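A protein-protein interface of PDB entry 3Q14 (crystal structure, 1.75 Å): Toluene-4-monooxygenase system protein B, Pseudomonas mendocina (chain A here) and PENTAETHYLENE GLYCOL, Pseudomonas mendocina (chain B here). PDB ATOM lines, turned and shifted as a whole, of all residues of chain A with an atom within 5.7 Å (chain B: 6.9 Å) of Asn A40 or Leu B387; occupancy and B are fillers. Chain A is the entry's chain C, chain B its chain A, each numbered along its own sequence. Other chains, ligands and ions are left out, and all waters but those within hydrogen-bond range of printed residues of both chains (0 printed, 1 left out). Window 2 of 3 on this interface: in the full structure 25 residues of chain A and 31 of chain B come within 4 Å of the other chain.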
ATOM      1  N   CYS A  38       9.505  23.471  15.673  1.00  0.00           N
ATOM      2  CA  CYS A  38       8.423  24.271  16.260  1.00  0.00           C
ATOM      3  C   CYS A  38       8.366  24.234  17.785  1.00  0.00           C
ATOM      4  O   CYS A  38       8.386  25.279  18.444  1.00  0.00           O
ATOM      5  CB  CYS A  38       7.074  23.824  15.698  1.00  0.00           C
ATOM      6  SG  CYS A  38       7.057  23.724  13.905  1.00  0.00           S
ATOM      7  N   VAL A  39       8.267  23.032  18.343  1.00  0.00           N
ATOM      8  CA  VAL A  39       8.158  22.866  19.785  1.00  0.00           C
ATOM      9  C   VAL A  39       9.440  23.341  20.474  1.00  0.00           C
ATOM     10  O   VAL A  39      10.548  23.027  20.038  1.00  0.00           O
ATOM     11  CB  VAL A  39       7.857  21.396  20.158  1.00  0.00           C
ATOM     12  CG1 VAL A  39       7.846  21.213  21.671  1.00  0.00           C
ATOM     13  CG2 VAL A  39       6.526  20.959  19.548  1.00  0.00           C
ATOM     14  N   ASN A  40       9.273  24.113  21.543  1.00  0.00           N
ATOM     15  CA  ASN A  40      10.391  24.693  22.272  1.00  0.00           C
ATOM     16  C   ASN A  40      11.135  25.762  21.476  1.00  0.00           C
ATOM     17  O   ASN A  40      12.199  26.208  21.877  1.00  0.00           O
ATOM     18  CB  ASN A  40      11.351  23.606  22.769  1.00  0.00           C
ATOM     19  CG  ASN A  40      10.716  22.708  23.813  1.00  0.00           C
ATOM     20  OD1 ASN A  40      10.019  23.181  24.711  1.00  0.00           O
ATOM     21  ND2 ASN A  40      10.946  21.406  23.695  1.00  0.00           N
ATOM     22  N   ARG A  41      10.573  26.164  20.340  1.00  0.00           N
ATOM     23  CA  ARG A  41      11.088  27.312  19.604  1.00  0.00           C
ATOM     24  C   ARG A  41      10.052  28.422  19.635  1.00  0.00           C
ATOM     25  O   ARG A  41      10.337  29.541  20.052  1.00  0.00           O
ATOM     26  CB  ARG A  41      11.410  26.952  18.155  1.00  0.00           C
ATOM     27  CG  ARG A  41      12.574  25.985  18.008  1.00  0.00           C
ATOM     28  CD  ARG A  41      12.776  25.589  16.559  1.00  0.00           C
ATOM     29  NE  ARG A  41      13.885  24.650  16.428  1.00  0.00           N
ATOM     30  CZ  ARG A  41      15.154  25.019  16.314  1.00  0.00           C
ATOM     31  NH1 ARG A  41      15.468  26.306  16.304  1.00  0.00           N
ATOM     32  NH2 ARG A  41      16.108  24.103  16.209  1.00  0.00           N
ATOM     33  N   ARG A  42       8.839  28.096  19.200  1.00  0.00           N
ATOM     34  CA  ARG A  42       7.760  29.071  19.201  1.00  0.00           C
ATOM     35  C   ARG A  42       6.491  28.478  19.794  1.00  0.00           C
ATOM     36  O   ARG A  42       5.506  29.188  20.000  1.00  0.00           O
ATOM     37  CB  ARG A  42       7.507  29.586  17.780  1.00  0.00           C
ATOM     38  CG  ARG A  42       8.705  30.293  17.170  1.00  0.00           C
ATOM     39  CD  ARG A  42       8.459  30.651  15.720  1.00  0.00           C
ATOM     40  NE  ARG A  42       8.105  29.466  14.949  1.00  0.00           N
ATOM     41  CZ  ARG A  42       8.991  28.636  14.407  1.00  0.00           C
ATOM     42  NH1 ARG A  42       8.579  27.574  13.733  1.00  0.00           N
ATOM     43  NH2 ARG A  42      10.293  28.866  14.544  1.00  0.00           N
ATOM     44  N   VAL A  43       6.529  27.180  20.082  1.00  0.00           N
ATOM     45  CA  VAL A  43       5.357  26.468  20.566  1.00  0.00           C
ATOM     46  C   VAL A  43       5.693  25.713  21.844  1.00  0.00           C
ATOM     47  O   VAL A  43       6.671  24.965  21.893  1.00  0.00           O
ATOM     48  CB  VAL A  43       4.832  25.472  19.514  1.00  0.00           C
ATOM     49  CG1 VAL A  43       3.743  24.594  20.110  1.00  0.00           C
ATOM     50  CG2 VAL A  43       4.309  26.226  18.295  1.00  0.00           C
ATOM     51  N   ALA A  44       4.877  25.914  22.872  1.00  0.00           N
ATOM     52  CA  ALA A  44       5.091  25.250  24.151  1.00  0.00           C
ATOM     53  C   ALA A  44       4.862  23.748  24.024  1.00  0.00           C
ATOM     54  O   ALA A  44       3.905  23.308  23.386  1.00  0.00           O
ATOM     55  CB  ALA A  44       4.178  25.841  25.212  1.00  0.00           C
ATOM     56  N   PRO A  45       5.750  22.950  24.627  1.00  0.00           N
ATOM     57  CA  PRO A  45       5.554  21.498  24.620  1.00  0.00           C
ATOM     58  C   PRO A  45       4.291  21.139  25.393  1.00  0.00           C
ATOM     59  O   PRO A  45       3.903  21.868  26.308  1.00  0.00           O
ATOM     60  CB  PRO A  45       6.796  20.974  25.342  1.00  0.00           C
ATOM     61  CG  PRO A  45       7.262  22.128  26.186  1.00  0.00           C
ATOM     62  CD  PRO A  45       6.942  23.354  25.394  1.00  0.00           C
ATOM     63  N   TYR B 337      12.682  35.932  13.580  1.00  0.00           N
ATOM     64  CA  TYR B 337      13.204  34.591  13.805  1.00  0.00           C
ATOM     65  C   TYR B 337      14.228  34.248  12.727  1.00  0.00           C
ATOM     66  O   TYR B 337      15.254  33.645  13.021  1.00  0.00           O
ATOM     67  CB  TYR B 337      12.081  33.544  13.860  1.00  0.00           C
ATOM     68  CG  TYR B 337      12.515  32.268  14.558  1.00  0.00           C
ATOM     69  CD1 TYR B 337      12.477  32.165  15.945  1.00  0.00           C
ATOM     70  CD2 TYR B 337      12.989  31.184  13.833  1.00  0.00           C
ATOM     71  CE1 TYR B 337      12.882  31.001  16.594  1.00  0.00           C
ATOM     72  CE2 TYR B 337      13.406  30.019  14.474  1.00  0.00           C
ATOM     73  CZ  TYR B 337      13.351  29.941  15.852  1.00  0.00           C
ATOM     74  OH  TYR B 337      13.756  28.791  16.497  1.00  0.00           O
ATOM     75  N   VAL B 375       7.804  31.632  24.608  1.00  0.00           N
ATOM     76  CA  VAL B 375       8.737  30.530  24.417  1.00  0.00           C
ATOM     77  C   VAL B 375      10.118  31.074  24.052  1.00  0.00           C
ATOM     78  O   VAL B 375      11.139  30.659  24.611  1.00  0.00           O
ATOM     79  CB  VAL B 375       8.246  29.559  23.322  1.00  0.00           C
ATOM     80  CG1 VAL B 375       9.265  28.456  23.098  1.00  0.00           C
ATOM     81  CG2 VAL B 375       6.877  28.985  23.693  1.00  0.00           C
ATOM     82  N   ILE B 376      10.138  32.018  23.120  1.00  0.00           N
ATOM     83  CA  ILE B 376      11.376  32.663  22.700  1.00  0.00           C
ATOM     84  C   ILE B 376      12.072  33.367  23.867  1.00  0.00           C
ATOM     85  O   ILE B 376      13.282  33.229  24.075  1.00  0.00           O
ATOM     86  CB  ILE B 376      11.098  33.693  21.592  1.00  0.00           C
ATOM     87  CG1 ILE B 376      10.688  32.972  20.297  1.00  0.00           C
ATOM     88  CG2 ILE B 376      12.318  34.565  21.371  1.00  0.00           C
ATOM     89  CD1 ILE B 376      10.020  33.878  19.275  1.00  0.00           C
ATOM     90  N   GLU B 378      11.730  32.829  27.088  1.00  0.00           N
ATOM     91  CA  GLU B 378      12.238  31.811  28.018  1.00  0.00           C
ATOM     92  C   GLU B 378      13.575  31.260  27.537  1.00  0.00           C
ATOM     93  O   GLU B 378      14.507  31.090  28.321  1.00  0.00           O
ATOM     94  CB  GLU B 378      11.258  30.644  28.163  1.00  0.00           C
ATOM     95  CG  GLU B 378       9.884  30.986  28.722  1.00  0.00           C
ATOM     96  CD  GLU B 378       8.847  29.889  28.437  1.00  0.00           C
ATOM     97  OE1 GLU B 378       9.245  28.716  28.246  1.00  0.00           O
ATOM     98  OE2 GLU B 378       7.634  30.200  28.391  1.00  0.00           O
ATOM     99  N   ASN B 379      13.655  30.952  26.246  1.00  0.00           N
ATOM    100  CA  ASN B 379      14.888  30.420  25.680  1.00  0.00           C
ATOM    101  C   ASN B 379      16.026  31.423  25.822  1.00  0.00           C
ATOM    102  O   ASN B 379      17.157  31.055  26.149  1.00  0.00           O
ATOM    103  CB  ASN B 379      14.700  30.030  24.208  1.00  0.00           C
ATOM    104  CG  ASN B 379      13.938  28.721  24.035  1.00  0.00           C
ATOM    105  OD1 ASN B 379      13.246  28.514  23.031  1.00  0.00           O
ATOM    106  ND2 ASN B 379      14.061  27.830  25.012  1.00  0.00           N
ATOM    107  N   ARG B 384      19.422  29.401  25.833  1.00  0.00           N
ATOM    108  CA  ARG B 384      19.237  28.360  24.824  1.00  0.00           C
ATOM    109  C   ARG B 384      19.162  29.001  23.438  1.00  0.00           C
ATOM    110  O   ARG B 384      18.115  28.965  22.782  1.00  0.00           O
ATOM    111  CB  ARG B 384      17.960  27.566  25.092  1.00  0.00           C
ATOM    112  CG  ARG B 384      17.752  27.142  26.538  1.00  0.00           C
ATOM    113  CD  ARG B 384      16.525  26.245  26.665  1.00  0.00           C
ATOM    114  NE  ARG B 384      16.060  26.134  28.045  1.00  0.00           N
ATOM    115  CZ  ARG B 384      14.946  26.692  28.509  1.00  0.00           C
ATOM    116  NH1 ARG B 384      14.166  27.395  27.700  1.00  0.00           N
ATOM    117  NH2 ARG B 384      14.606  26.541  29.784  1.00  0.00           N
ATOM    118  N   MET B 385      20.277  29.572  22.991  1.00  0.00           N
ATOM    119  CA  MET B 385      20.279  30.409  21.788  1.00  0.00           C
ATOM    120  C   MET B 385      20.083  29.637  20.490  1.00  0.00           C
ATOM    121  O   MET B 385      19.642  30.202  19.487  1.00  0.00           O
ATOM    122  CB  MET B 385      21.542  31.270  21.715  1.00  0.00           C
ATOM    123  CG  MET B 385      21.701  32.231  22.889  1.00  0.00           C
ATOM    124  SD  MET B 385      20.212  33.203  23.228  1.00  0.00           S
ATOM    125  CE  MET B 385      20.177  34.253  21.784  1.00  0.00           C
ATOM    126  N   ASP B 386      20.402  28.349  20.499  1.00  0.00           N
ATOM    127  CA  ASP B 386      20.157  27.527  19.320  1.00  0.00           C
ATOM    128  C   ASP B 386      18.663  27.455  18.980  1.00  0.00           C
ATOM    129  O   ASP B 386      18.298  27.265  17.824  1.00  0.00           O
ATOM    130  CB  ASP B 386      20.722  26.119  19.513  1.00  0.00           C
ATOM    131  CG  ASP B 386      20.126  25.418  20.711  1.00  0.00           C
ATOM    132  OD1 ASP B 386      19.554  24.324  20.532  1.00  0.00           O
ATOM    133  OD2 ASP B 386      20.233  25.963  21.834  1.00  0.00           O
ATOM    134  N   LEU B 387      17.805  27.613  19.985  1.00  0.00           N
ATOM    135  CA  LEU B 387      16.359  27.529  19.778  1.00  0.00           C
ATOM    136  C   LEU B 387      15.764  28.846  19.273  1.00  0.00           C
ATOM    137  O   LEU B 387      14.560  28.929  19.002  1.00  0.00           O
ATOM    138  CB  LEU B 387      15.649  27.093  21.063  1.00  0.00           C
ATOM    139  CG  LEU B 387      16.051  25.715  21.595  1.00  0.00           C
ATOM    140  CD1 LEU B 387      15.255  25.363  22.852  1.00  0.00           C
ATOM    141  CD2 LEU B 387      15.855  24.667  20.518  1.00  0.00           C
ATOM    142  N   VAL B 388      16.604  29.870  19.148  1.00  0.00           N
ATOM    143  CA  VAL B 388      16.153  31.158  18.619  1.00  0.00           C
ATOM    144  C   VAL B 388      16.714  31.445  17.224  1.00  0.00           C
ATOM    145  O   VAL B 388      16.678  32.582  16.747  1.00  0.00           O
ATOM    146  CB  VAL B 388      16.501  32.324  19.568  1.00  0.00           C
ATOM    147  CG1 VAL B 388      15.970  32.045  20.963  1.00  0.00           C
ATOM    148  CG2 VAL B 388      17.997  32.569  19.589  1.00  0.00           C
ATOM    149  N   SER B 389      17.229  30.406  16.576  1.00  0.00           N
ATOM    150  CA  SER B 389      17.684  30.502  15.194  1.00  0.00           C
ATOM    151  C   SER B 389      17.145  29.300  14.426  1.00  0.00           C
ATOM    152  O   SER B 389      17.122  28.187  14.950  1.00  0.00           O
ATOM    153  CB  SER B 389      19.204  30.539  15.126  1.00  0.00           C
ATOM    154  OG  SER B 389      19.706  31.672  15.811  1.00  0.00           O
ATOM    155  N   PRO B 390      16.709  29.523  13.178  1.00  0.00           N
ATOM    156  CA  PRO B 390      16.033  28.473  12.415  1.00  0.00           C
ATOM    157  C   PRO B 390      16.977  27.459  11.779  1.00  0.00           C
ATOM    158  O   PRO B 390      18.147  27.743  11.487  1.00  0.00           O
ATOM    159  CB  PRO B 390      15.317  29.261  11.317  1.00  0.00           C
ATOM    160  CG  PRO B 390      16.256  30.408  11.060  1.00  0.00           C
ATOM    161  CD  PRO B 390      16.823  30.777  12.413  1.00  0.00           C
ATOM    162  N   GLU B 391      16.450  26.266  11.547  1.00  0.00           N
ATOM    163  CA  GLU B 391      17.211  25.222  10.876  1.00  0.00           C
ATOM    164  C   GLU B 391      16.462  24.713   9.657  1.00  0.00           C
ATOM    165  O   GLU B 391      16.780  23.662   9.110  1.00  0.00           O
ATOM    166  CB  GLU B 391      17.527  24.088  11.847  1.00  0.00           C
ATOM    167  CG  GLU B 391      18.454  24.530  12.963  1.00  0.00           C
ATOM    168  CD  GLU B 391      18.601  23.485  14.050  1.00  0.00           C
ATOM    169  OE1 GLU B 391      18.712  22.285  13.717  1.00  0.00           O
ATOM    170  OE2 GLU B 391      18.598  23.870  15.239  1.00  0.00           O
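OH of Tyr B337 lies within hydrogen-bond range of NH1 of Arg A41 (3.0 Å).
The backbone carbonyl oxygen (O) of Asn A40 sits close to the side-chain amide oxygen (OD1) of Asn B379, 2.8 Å away.
OE2 of Glu B391 is in salt-bridge range of NH2 of Arg A41.
The guanidinium group (NH1) of Arg A41 lies within hydrogen-bond range of the backbone carbonyl oxygen (O) of Ser B389.
The backbone carbonyl oxygen of Asp B386 sits at hydrogen-bond distance from the guanidinium group of Arg A41 (3.4 Å).
The side-chain amide nitrogen (ND2) of Asn B379 lies close to the guanidinium group (NH1) of Arg B384 (2.7 Å).
The backbone carbonyl oxygen (O) of Cys A38 sits at hydrogen-bond distance from the backbone NH (N) of Val A43, 3.1 Å away.
The backbone carbonyl oxygen (O) of Val B375 sits close to the side-chain amide oxygen (OD1) of Asn B379, 3.4 Å away.
O of Leu B387 sits at hydrogen-bond distance from OH of Tyr B337 (2.6 Å).
Asn A40 touches Val B375.
Asn A40 touches Leu B387.
Arg A41 touches Val B375.
Arg A41 touches Ile B376.
Arg A41 touches Leu B387 (CG to O, 3.7 Å).
NH2 of Arg A42 touches CE2 of Tyr B337, 3.3 Å away.
CG1 of Val B375 touches N of Arg A42, 3.9 Å away.
Val A43 touches Val B375 (C to CG2, 3.9 Å).
N of Ala A44 touches CG2 of Val B375 (3.8 Å).
Asn A40 touches just these residues of chain B: Val B375, Asn B379 and Leu B387.
Of the printed residues of chain A, Leu B387 touches Asn A40 and Arg A41.
Of the printed residues of chain A, Asn B379 touches Asn A40 (2.8 Å).
Of the printed residues of chain A, Val B375 touches Asn A40 (3.7 Å), Arg A41 (3.4 Å), Arg A42 (3.9 Å), Val A43 (3.9 Å) and Ala A44 (3.8 Å).
The nearest residue of chain B that does not touch Asn A40 is Tyr B337 (6.2 Å).
The nearest residue of chain A that does not touch Leu B387 is Val A39 (5.6 Å).
Hydrophobic or aromatic side chains of chain B that line the printed part of chain A: Tyr B337, Val B375, Ile B376 and Leu B387.
Printed residues of chain A that touch a printed residue of chain B: Asn A40, Arg A41, Arg A42, Val A43 and Ala A44.
Along chain A the printed residues that touch a printed residue of chain B span positions 40 to 44.
Among the printed residues, 14 pairs touch across the chains.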
